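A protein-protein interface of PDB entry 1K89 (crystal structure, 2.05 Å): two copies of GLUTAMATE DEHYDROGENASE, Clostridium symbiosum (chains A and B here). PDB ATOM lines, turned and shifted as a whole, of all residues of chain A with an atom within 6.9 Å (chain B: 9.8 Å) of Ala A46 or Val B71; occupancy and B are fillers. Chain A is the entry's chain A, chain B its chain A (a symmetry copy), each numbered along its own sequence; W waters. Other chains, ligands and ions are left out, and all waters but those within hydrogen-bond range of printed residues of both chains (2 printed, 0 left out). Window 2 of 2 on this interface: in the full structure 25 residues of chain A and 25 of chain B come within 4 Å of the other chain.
Water W1 lies within hydrogen-bond range of the backbone carbonyl oxygen of Glu A44 (2.4 Å) and the backbone NH of Val B71 (2.7 Å).
Water W2 lies within hydrogen-bond range of the guanidinium group (NH1) of Arg B61 and the side-chain sulfur (SD) of Met A442.
Val A45 touches Val B71.
Val B71 touches Ala A46 (O to CB, 3.7 Å).
Glu A49 touches Val B73 (CB to CG2, 3.9 Å).
Arg A50 touches Pro B63 (CD to CB, 3.9 Å).
CG of Arg A50 touches CG2 of Val B73 (3.6 Å).
Met A442 touches Arg B61.
OE1 of Glu A49 sits at hydrogen-bond distance from OH of Tyr A3.
NH2 of Arg A6 is in salt-bridge range of OE2 of Glu A49 (3.1 Å).
NH2 of Arg A50 sits at hydrogen-bond distance from O of Val A45, at 2.9 Å.
The guanidinium group of Arg B61 sits at hydrogen-bond distance from the backbone carbonyl oxygen of Arg A50 (2.8 Å).
No position is printed for both chains.
Of the 7 pairs that touch across the chains among the printed residues, none has its exchanged pair printed and touching as well.
Glu A41 touches none of the printed residues of chain B.
Printed residues of chain B within 4 Å of Val A45: Val B71.
Ala A46 touches just one residue of chain B: Val B71.
Printed residues of chain B within 4 Å of Glu A49: Val B73.
Printed residues of chain A within 4 Å of Arg B61: Arg A50 (2.8 Å) and Met A442 (3.8 Å).
Of the printed residues of chain A, Pro B63 touches Arg A50 (3.9 Å).
Of the printed residues of chain A, Val B71 touches Val A45 and Ala A46.
Of the printed residues of chain A, Val B73 touches Glu A49 and Arg A50.
The nearest residue of chain B that does not touch Ala A46 is Val B73 (4.4 Å).
The nearest printed residue of chain A that does not touch Pro B63 is Ile A447 (4.2 Å).
Of the 15 printed residues of chain A, 5 touch a printed residue of chain B.
Hydrophobic or aromatic side chains of chain A that line the printed part of chain B: Ala A46 and Met A442.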
ATOM      1  N   TYR A   3      24.442   5.716  26.476  1.00  0.00           N
ATOM      2  CA  TYR A   3      23.899   6.456  25.321  1.00  0.00           C
ATOM      3  C   TYR A   3      22.995   5.505  24.547  1.00  0.00           C
ATOM      4  O   TYR A   3      21.838   5.781  24.287  1.00  0.00           O
ATOM      5  CB  TYR A   3      25.057   6.898  24.435  1.00  0.00           C
ATOM      6  CG  TYR A   3      24.667   7.589  23.128  1.00  0.00           C
ATOM      7  CD1 TYR A   3      23.462   8.301  23.003  1.00  0.00           C
ATOM      8  CD2 TYR A   3      25.531   7.547  22.010  1.00  0.00           C
ATOM      9  CE1 TYR A   3      23.112   8.955  21.773  1.00  0.00           C
ATOM     10  CE2 TYR A   3      25.204   8.239  20.775  1.00  0.00           C
ATOM     11  CZ  TYR A   3      24.007   8.914  20.671  1.00  0.00           C
ATOM     12  OH  TYR A   3      23.747   9.578  19.481  1.00  0.00           O
ATOM     13  N   ARG A   6      19.909   4.866  26.515  1.00  0.00           N
ATOM     14  CA  ARG A   6      18.937   5.965  26.472  1.00  0.00           C
ATOM     15  C   ARG A   6      18.105   6.009  25.147  1.00  0.00           C
ATOM     16  O   ARG A   6      16.873   6.256  25.139  1.00  0.00           O
ATOM     17  CB  ARG A   6      19.696   7.279  26.728  1.00  0.00           C
ATOM     18  CG  ARG A   6      18.969   8.536  26.343  1.00  0.00           C
ATOM     19  CD  ARG A   6      19.751   9.800  26.766  1.00  0.00           C
ATOM     20  NE  ARG A   6      20.882  10.129  25.887  1.00  0.00           N
ATOM     21  CZ  ARG A   6      20.775  10.485  24.605  1.00  0.00           C
ATOM     22  NH1 ARG A   6      19.579  10.523  23.982  1.00  0.00           N
ATOM     23  NH2 ARG A   6      21.884  10.784  23.946  1.00  0.00           N
ATOM     24  N   GLU A  41      32.248  10.957  19.912  1.00  0.00           N
ATOM     25  CA  GLU A  41      31.845  11.951  18.946  1.00  0.00           C
ATOM     26  C   GLU A  41      30.447  11.669  18.399  1.00  0.00           C
ATOM     27  O   GLU A  41      29.707  12.581  18.030  1.00  0.00           O
ATOM     28  CB  GLU A  41      32.866  12.015  17.787  1.00  0.00           C
ATOM     29  CG  GLU A  41      32.791  10.887  16.801  1.00  0.00           C
ATOM     30  CD  GLU A  41      33.800   9.837  17.134  1.00  0.00           C
ATOM     31  OE1 GLU A  41      34.177   9.836  18.310  1.00  0.00           O
ATOM     32  OE2 GLU A  41      34.301   9.109  16.240  1.00  0.00           O
ATOM     33  N   TYR A  42      30.055  10.403  18.348  1.00  0.00           N
ATOM     34  CA  TYR A  42      28.708  10.113  17.839  1.00  0.00           C
ATOM     35  C   TYR A  42      27.612  10.818  18.604  1.00  0.00           C
ATOM     36  O   TYR A  42      26.677  11.417  18.047  1.00  0.00           O
ATOM     37  CB  TYR A  42      28.434   8.611  17.871  1.00  0.00           C
ATOM     38  CG  TYR A  42      29.357   7.794  17.000  1.00  0.00           C
ATOM     39  CD1 TYR A  42      30.147   8.399  16.036  1.00  0.00           C
ATOM     40  CD2 TYR A  42      29.338   6.394  17.062  1.00  0.00           C
ATOM     41  CE1 TYR A  42      30.888   7.647  15.176  1.00  0.00           C
ATOM     42  CE2 TYR A  42      30.114   5.640  16.213  1.00  0.00           C
ATOM     43  CZ  TYR A  42      30.872   6.272  15.279  1.00  0.00           C
ATOM     44  OH  TYR A  42      31.661   5.517  14.448  1.00  0.00           O
ATOM     45  N   GLU A  43      27.691  10.705  19.911  1.00  0.00           N
ATOM     46  CA  GLU A  43      26.674  11.285  20.746  1.00  0.00           C
ATOM     47  C   GLU A  43      26.612  12.793  20.587  1.00  0.00           C
ATOM     48  O   GLU A  43      25.521  13.418  20.691  1.00  0.00           O
ATOM     49  CB  GLU A  43      26.917  10.877  22.231  1.00  0.00           C
ATOM     50  CG  GLU A  43      25.913  11.534  23.180  1.00  0.00           C
ATOM     51  CD  GLU A  43      25.942  10.973  24.620  1.00  0.00           C
ATOM     52  OE1 GLU A  43      26.965  10.351  24.945  1.00  0.00           O
ATOM     53  OE2 GLU A  43      24.962  11.158  25.413  1.00  0.00           O
ATOM     54  N   GLU A  44      27.774  13.407  20.377  1.00  0.00           N
ATOM     55  CA  GLU A  44      27.794  14.877  20.245  1.00  0.00           C
ATOM     56  C   GLU A  44      26.956  15.374  19.053  1.00  0.00           C
ATOM     57  O   GLU A  44      26.509  16.513  19.053  1.00  0.00           O
ATOM     58  CB  GLU A  44      29.240  15.420  20.135  1.00  0.00           C
ATOM     59  CG  GLU A  44      30.069  15.487  21.457  1.00  0.00           C
ATOM     60  CD  GLU A  44      31.590  15.348  21.229  1.00  0.00           C
ATOM     61  OE1 GLU A  44      32.102  15.967  20.267  1.00  0.00           O
ATOM     62  OE2 GLU A  44      32.272  14.615  22.001  1.00  0.00           O
ATOM     63  N   VAL A  45      26.771  14.538  18.029  1.00  0.00           N
ATOM     64  CA  VAL A  45      25.986  14.929  16.842  1.00  0.00           C
ATOM     65  C   VAL A  45      24.664  14.161  16.778  1.00  0.00           C
ATOM     66  O   VAL A  45      23.985  14.199  15.744  1.00  0.00           O
ATOM     67  CB  VAL A  45      26.775  14.868  15.501  1.00  0.00           C
ATOM     68  CG1 VAL A  45      27.934  15.894  15.507  1.00  0.00           C
ATOM     69  CG2 VAL A  45      27.332  13.501  15.272  1.00  0.00           C
ATOM     70  N   ALA A  46      24.296  13.518  17.904  1.00  0.00           N
ATOM     71  CA  ALA A  46      23.024  12.801  18.011  1.00  0.00           C
ATOM     72  C   ALA A  46      22.886  11.788  16.860  1.00  0.00           C
ATOM     73  O   ALA A  46      21.832  11.643  16.200  1.00  0.00           O
ATOM     74  CB  ALA A  46      21.900  13.767  17.981  1.00  0.00           C
ATOM     75  N   LEU A  47      23.988  11.106  16.611  1.00  0.00           N
ATOM     76  CA  LEU A  47      24.026  10.134  15.533  1.00  0.00           C
ATOM     77  C   LEU A  47      22.916   9.083  15.641  1.00  0.00           C
ATOM     78  O   LEU A  47      22.236   8.787  14.666  1.00  0.00           O
ATOM     79  CB  LEU A  47      25.426   9.446  15.463  1.00  0.00           C
ATOM     80  CG  LEU A  47      25.559   8.476  14.268  1.00  0.00           C
ATOM     81  CD1 LEU A  47      25.415   9.233  12.982  1.00  0.00           C
ATOM     82  CD2 LEU A  47      26.794   7.581  14.197  1.00  0.00           C
ATOM     83  N   LEU A  48      22.771   8.463  16.805  1.00  0.00           N
ATOM     84  CA  LEU A  48      21.783   7.391  16.935  1.00  0.00           C
ATOM     85  C   LEU A  48      20.369   7.911  16.862  1.00  0.00           C
ATOM     86  O   LEU A  48      19.487   7.243  16.321  1.00  0.00           O
ATOM     87  CB  LEU A  48      21.982   6.624  18.256  1.00  0.00           C
ATOM     88  CG  LEU A  48      23.266   5.816  18.421  1.00  0.00           C
ATOM     89  CD1 LEU A  48      23.137   4.950  19.698  1.00  0.00           C
ATOM     90  CD2 LEU A  48      23.529   4.943  17.207  1.00  0.00           C
ATOM     91  N   GLU A  49      20.155   9.107  17.421  1.00  0.00           N
ATOM     92  CA  GLU A  49      18.832   9.660  17.422  1.00  0.00           C
ATOM     93  C   GLU A  49      18.425   9.944  15.976  1.00  0.00           C
ATOM     94  O   GLU A  49      17.274   9.802  15.603  1.00  0.00           O
ATOM     95  CB  GLU A  49      18.777  10.943  18.242  1.00  0.00           C
ATOM     96  CG  GLU A  49      19.006  10.757  19.721  1.00  0.00           C
ATOM     97  CD  GLU A  49      20.467  10.908  20.065  1.00  0.00           C
ATOM     98  OE1 GLU A  49      21.339  10.468  19.290  1.00  0.00           O
ATOM     99  OE2 GLU A  49      20.752  11.420  21.153  1.00  0.00           O
ATOM    100  N   ARG A  50      19.361  10.386  15.162  1.00  0.00           N
ATOM    101  CA  ARG A  50      19.050  10.617  13.748  1.00  0.00           C
ATOM    102  C   ARG A  50      18.770   9.288  13.011  1.00  0.00           C
ATOM    103  O   ARG A  50      17.869   9.198  12.204  1.00  0.00           O
ATOM    104  CB  ARG A  50      20.277  11.273  13.093  1.00  0.00           C
ATOM    105  CG  ARG A  50      20.355  12.779  13.380  1.00  0.00           C
ATOM    106  CD  ARG A  50      21.201  13.372  12.300  1.00  0.00           C
ATOM    107  NE  ARG A  50      22.486  13.462  12.866  1.00  0.00           N
ATOM    108  CZ  ARG A  50      23.649  13.452  12.240  1.00  0.00           C
ATOM    109  NH1 ARG A  50      23.752  13.473  10.920  1.00  0.00           N
ATOM    110  NH2 ARG A  50      24.735  13.508  13.009  1.00  0.00           N
ATOM    111  N   MET A  51      19.624   8.297  13.239  1.00  0.00           N
ATOM    112  CA  MET A  51      19.489   7.021  12.552  1.00  0.00           C
ATOM    113  C   MET A  51      18.183   6.312  12.760  1.00  0.00           C
ATOM    114  O   MET A  51      17.772   5.533  11.914  1.00  0.00           O
ATOM    115  CB  MET A  51      20.620   6.025  12.896  1.00  0.00           C
ATOM    116  CG  MET A  51      22.008   6.496  12.483  1.00  0.00           C
ATOM    117  SD  MET A  51      23.264   5.197  12.608  1.00  0.00           S
ATOM    118  CE  MET A  51      22.191   3.905  12.328  1.00  0.00           C
ATOM    119  N   MET A 442      27.773   9.194   7.602  1.00  0.00           N
ATOM    120  CA  MET A 442      26.999  10.257   8.228  1.00  0.00           C
ATOM    121  C   MET A 442      27.861  11.296   8.943  1.00  0.00           C
ATOM    122  O   MET A 442      27.563  12.511   8.895  1.00  0.00           O
ATOM    123  CB  MET A 442      25.924   9.673   9.210  1.00  0.00           C
ATOM    124  CG  MET A 442      24.902   8.776   8.473  1.00  0.00           C
ATOM    125  SD  MET A 442      23.520   8.282   9.404  1.00  0.00           S
ATOM    126  CE  MET A 442      22.729   9.806   9.991  1.00  0.00           C
ATOM    127  N   ILE A 447      25.500  17.432   9.590  1.00  0.00           N
ATOM    128  CA  ILE A 447      24.178  17.493  10.103  1.00  0.00           C
ATOM    129  C   ILE A 447      23.344  18.169   9.058  1.00  0.00           C
ATOM    130  O   ILE A 447      23.251  19.383   9.045  1.00  0.00           O
ATOM    131  CB  ILE A 447      24.223  18.433  11.346  1.00  0.00           C
ATOM    132  CG1 ILE A 447      25.231  17.864  12.377  1.00  0.00           C
ATOM    133  CG2 ILE A 447      22.902  18.520  11.982  1.00  0.00           C
ATOM    134  CD1 ILE A 447      25.488  16.388  12.162  1.00  0.00           C
ATOM    135  N   ARG B  61      12.670  13.329   8.669  1.00  0.00           N
ATOM    136  CA  ARG B  61      13.549  13.625   9.797  1.00  0.00           C
ATOM    137  C   ARG B  61      13.907  15.088   9.811  1.00  0.00           C
ATOM    138  O   ARG B  61      14.154  15.663   8.745  1.00  0.00           O
ATOM    139  CB  ARG B  61      14.831  12.784   9.593  1.00  0.00           C
ATOM    140  CG  ARG B  61      15.796  12.864  10.731  1.00  0.00           C
ATOM    141  CD  ARG B  61      17.093  12.242  10.491  1.00  0.00           C
ATOM    142  NE  ARG B  61      17.020  10.864  10.083  1.00  0.00           N
ATOM    143  CZ  ARG B  61      18.017  10.246   9.444  1.00  0.00           C
ATOM    144  NH1 ARG B  61      19.174  10.890   9.164  1.00  0.00           N
ATOM    145  NH2 ARG B  61      17.882   8.972   9.069  1.00  0.00           N
ATOM    146  N   VAL B  62      14.019  15.688  10.994  1.00  0.00           N
ATOM    147  CA  VAL B  62      14.446  17.076  11.071  1.00  0.00           C
ATOM    148  C   VAL B  62      15.501  17.306  12.145  1.00  0.00           C
ATOM    149  O   VAL B  62      15.146  17.639  13.289  1.00  0.00           O
ATOM    150  CB  VAL B  62      13.291  18.081  11.296  1.00  0.00           C
ATOM    151  CG1 VAL B  62      13.809  19.585  11.088  1.00  0.00           C
ATOM    152  CG2 VAL B  62      12.105  17.773  10.350  1.00  0.00           C
ATOM    153  N   PRO B  63      16.772  17.190  11.760  1.00  0.00           N
ATOM    154  CA  PRO B  63      17.898  17.460  12.687  1.00  0.00           C
ATOM    155  C   PRO B  63      18.175  18.939  12.610  1.00  0.00           C
ATOM    156  O   PRO B  63      18.022  19.561  11.560  1.00  0.00           O
ATOM    157  CB  PRO B  63      19.107  16.699  12.104  1.00  0.00           C
ATOM    158  CG  PRO B  63      18.607  16.060  10.785  1.00  0.00           C
ATOM    159  CD  PRO B  63      17.199  16.562  10.490  1.00  0.00           C
ATOM    160  N   TRP B  64      18.524  19.508  13.752  1.00  0.00           N
ATOM    161  CA  TRP B  64      18.843  20.924  13.846  1.00  0.00           C
ATOM    162  C   TRP B  64      19.752  21.197  15.064  1.00  0.00           C
ATOM    163  O   TRP B  64      19.802  20.408  16.008  1.00  0.00           O
ATOM    164  CB  TRP B  64      17.573  21.720  13.915  1.00  0.00           C
ATOM    165  CG  TRP B  64      16.725  21.375  15.047  1.00  0.00           C
ATOM    166  CD1 TRP B  64      15.836  20.340  15.160  1.00  0.00           C
ATOM    167  CD2 TRP B  64      16.643  22.131  16.253  1.00  0.00           C
ATOM    168  NE1 TRP B  64      15.180  20.434  16.383  1.00  0.00           N
ATOM    169  CE2 TRP B  64      15.750  21.463  17.104  1.00  0.00           C
ATOM    170  CE3 TRP B  64      17.304  23.288  16.715  1.00  0.00           C
ATOM    171  CZ2 TRP B  64      15.457  21.943  18.395  1.00  0.00           C
ATOM    172  CZ3 TRP B  64      17.039  23.741  18.006  1.00  0.00           C
ATOM    173  CH2 TRP B  64      16.104  23.086  18.820  1.00  0.00           C
ATOM    174  N   GLU B  65      20.504  22.289  15.036  1.00  0.00           N
ATOM    175  CA  GLU B  65      21.424  22.589  16.136  1.00  0.00           C
ATOM    176  C   GLU B  65      20.935  23.765  16.971  1.00  0.00           C
ATOM    177  O   GLU B  65      20.360  24.762  16.435  1.00  0.00           O
ATOM    178  CB  GLU B  65      22.883  22.740  15.611  1.00  0.00           C
ATOM    179  CG  GLU B  65      23.523  24.061  15.674  1.00  0.00           C
ATOM    180  CD  GLU B  65      24.854  24.062  14.945  1.00  0.00           C
ATOM    181  OE1 GLU B  65      25.874  23.732  15.587  1.00  0.00           O
ATOM    182  OE2 GLU B  65      24.875  24.396  13.728  1.00  0.00           O
ATOM    183  N   ASP B  66      21.086  23.661  18.296  1.00  0.00           N
ATOM    184  CA  ASP B  66      20.629  24.797  19.095  1.00  0.00           C
ATOM    185  C   ASP B  66      21.754  25.796  19.247  1.00  0.00           C
ATOM    186  O   ASP B  66      22.866  25.602  18.716  1.00  0.00           O
ATOM    187  CB  ASP B  66      20.087  24.382  20.457  1.00  0.00           C
ATOM    188  CG  ASP B  66      21.141  23.708  21.340  1.00  0.00           C
ATOM    189  OD1 ASP B  66      22.392  23.894  21.239  1.00  0.00           O
ATOM    190  OD2 ASP B  66      20.658  22.974  22.204  1.00  0.00           O
ATOM    191  N   ASP B  67      21.449  26.856  19.990  1.00  0.00           N
ATOM    192  CA  ASP B  67      22.392  27.964  20.239  1.00  0.00           C
ATOM    193  C   ASP B  67      23.664  27.485  20.959  1.00  0.00           C
ATOM    194  O   ASP B  67      24.704  28.090  20.812  1.00  0.00           O
ATOM    195  CB  ASP B  67      21.682  29.050  21.054  1.00  0.00           C
ATOM    196  CG  ASP B  67      20.784  29.897  20.214  1.00  0.00           C
ATOM    197  OD1 ASP B  67      20.843  29.728  18.986  1.00  0.00           O
ATOM    198  OD2 ASP B  67      19.963  30.694  20.741  1.00  0.00           O
ATOM    199  N   ASN B  68      23.570  26.379  21.708  1.00  0.00           N
ATOM    200  CA  ASN B  68      24.705  25.780  22.386  1.00  0.00           C
ATOM    201  C   ASN B  68      25.431  24.793  21.526  1.00  0.00           C
ATOM    202  O   ASN B  68      26.401  24.243  21.975  1.00  0.00           O
ATOM    203  CB  ASN B  68      24.245  25.071  23.640  1.00  0.00           C
ATOM    204  CG  ASN B  68      23.695  26.041  24.658  1.00  0.00           C
ATOM    205  OD1 ASN B  68      22.613  25.842  25.205  1.00  0.00           O
ATOM    206  ND2 ASN B  68      24.372  27.176  24.803  1.00  0.00           N
ATOM    207  N   GLY B  69      24.998  24.559  20.288  1.00  0.00           N
ATOM    208  CA  GLY B  69      25.762  23.638  19.455  1.00  0.00           C
ATOM    209  C   GLY B  69      25.250  22.242  19.676  1.00  0.00           C
ATOM    210  O   GLY B  69      25.748  21.315  19.075  1.00  0.00           O
ATOM    211  N   LYS B  70      24.208  22.065  20.466  1.00  0.00           N
ATOM    212  CA  LYS B  70      23.765  20.690  20.636  1.00  0.00           C
ATOM    213  C   LYS B  70      22.825  20.328  19.501  1.00  0.00           C
ATOM    214  O   LYS B  70      22.043  21.139  19.105  1.00  0.00           O
ATOM    215  CB  LYS B  70      23.057  20.510  21.972  1.00  0.00           C
ATOM    216  CG  LYS B  70      21.907  19.531  21.896  1.00  0.00           C
ATOM    217  CD  LYS B  70      21.663  18.841  23.250  1.00  0.00           C
ATOM    218  CE  LYS B  70      21.150  17.390  23.108  1.00  0.00           C
ATOM    219  NZ  LYS B  70      20.118  17.003  24.137  1.00  0.00           N
ATOM    220  N   VAL B  71      22.885  19.082  19.040  1.00  0.00           N
ATOM    221  CA  VAL B  71      22.025  18.607  17.971  1.00  0.00           C
ATOM    222  C   VAL B  71      20.748  17.934  18.464  1.00  0.00           C
ATOM    223  O   VAL B  71      20.786  17.047  19.308  1.00  0.00           O
ATOM    224  CB  VAL B  71      22.821  17.657  17.097  1.00  0.00           C
ATOM    225  CG1 VAL B  71      21.942  17.044  15.917  1.00  0.00           C
ATOM    226  CG2 VAL B  71      23.980  18.462  16.517  1.00  0.00           C
ATOM    227  N   HIS B  72      19.615  18.391  17.945  1.00  0.00           N
ATOM    228  CA  HIS B  72      18.298  17.837  18.242  1.00  0.00           C
ATOM    229  C   HIS B  72      17.672  17.238  16.986  1.00  0.00           C
ATOM    230  O   HIS B  72      18.033  17.591  15.856  1.00  0.00           O
ATOM    231  CB  HIS B  72      17.406  18.942  18.724  1.00  0.00           C
ATOM    232  CG  HIS B  72      17.941  19.628  19.941  1.00  0.00           C
ATOM    233  ND1 HIS B  72      17.565  19.270  21.216  1.00  0.00           N
ATOM    234  CD2 HIS B  72      18.887  20.586  20.083  1.00  0.00           C
ATOM    235  CE1 HIS B  72      18.224  20.005  22.094  1.00  0.00           C
ATOM    236  NE2 HIS B  72      19.035  20.811  21.435  1.00  0.00           N
ATOM    237  N   VAL B  73      16.761  16.303  17.175  1.00  0.00           N
ATOM    238  CA  VAL B  73      16.095  15.646  16.048  1.00  0.00           C
ATOM    239  C   VAL B  73      14.598  15.603  16.237  1.00  0.00           C
ATOM    240  O   VAL B  73      14.144  15.019  17.188  1.00  0.00           O
ATOM    241  CB  VAL B  73      16.557  14.161  15.817  1.00  0.00           C
ATOM    242  CG1 VAL B  73      16.150  13.750  14.372  1.00  0.00           C
ATOM    243  CG2 VAL B  73      18.064  14.014  15.906  1.00  0.00           C
ATOM    244  N   ASN B  74      13.839  16.210  15.337  1.00  0.00           N
ATOM    245  CA  ASN B  74      12.415  16.128  15.412  1.00  0.00           C
ATOM    246  C   ASN B  74      11.888  15.493  14.123  1.00  0.00           C
ATOM    247  O   ASN B  74      12.655  15.124  13.232  1.00  0.00           O
ATOM    248  CB  ASN B  74      11.810  17.498  15.666  1.00  0.00           C
ATOM    249  CG  ASN B  74      12.119  17.979  17.056  1.00  0.00           C
ATOM    250  OD1 ASN B  74      13.146  18.606  17.312  1.00  0.00           O
ATOM    251  ND2 ASN B  74      11.277  17.603  17.987  1.00  0.00           N
ATOM    252  N   GLU B 139      17.148  29.787  17.242  1.00  0.00           N
ATOM    253  CA  GLU B 139      16.890  28.341  17.215  1.00  0.00           C
ATOM    254  C   GLU B 139      15.632  28.022  16.352  1.00  0.00           C
ATOM    255  O   GLU B 139      15.611  27.102  15.566  1.00  0.00           O
ATOM    256  CB  GLU B 139      16.720  27.806  18.628  1.00  0.00           C
ATOM    257  CG  GLU B 139      18.066  27.769  19.348  1.00  0.00           C
ATOM    258  CD  GLU B 139      17.966  27.502  20.880  1.00  0.00           C
ATOM    259  OE1 GLU B 139      16.899  27.779  21.495  1.00  0.00           O
ATOM    260  OE2 GLU B 139      19.019  27.098  21.430  1.00  0.00           O
ATOM    261  N   ARG B 142      16.710  28.197  12.665  1.00  0.00           N
ATOM    262  CA  ARG B 142      17.480  27.085  12.180  1.00  0.00           C
ATOM    263  C   ARG B 142      16.539  25.906  12.003  1.00  0.00           C
ATOM    264  O   ARG B 142      16.693  25.132  11.072  1.00  0.00           O
ATOM    265  CB  ARG B 142      18.665  26.768  13.121  1.00  0.00           C
ATOM    266  CG  ARG B 142      19.761  27.833  13.032  1.00  0.00           C
ATOM    267  CD  ARG B 142      21.160  27.362  13.511  1.00  0.00           C
ATOM    268  NE  ARG B 142      21.013  27.166  14.888  1.00  0.00           N
ATOM    269  CZ  ARG B 142      21.272  28.063  15.822  1.00  0.00           C
ATOM    270  NH1 ARG B 142      21.880  29.228  15.593  1.00  0.00           N
ATOM    271  NH2 ARG B 142      20.967  27.700  17.055  1.00  0.00           N
ATOM    272  N   ALA B 146      15.755  23.943   8.470  1.00  0.00           N
ATOM    273  CA  ALA B 146      16.017  22.508   8.298  1.00  0.00           C
ATOM    274  C   ALA B 146      14.705  21.842   7.830  1.00  0.00           C
ATOM    275  O   ALA B 146      14.738  20.942   6.981  1.00  0.00           O
ATOM    276  CB  ALA B 146      16.462  21.864   9.608  1.00  0.00           C
HETATM  277  O   HOH W   1      24.531  17.302  20.163  1.00  0.00           O
HETATM  278  O   HOH W   2      20.587   8.911   7.371  1.00  0.00           O
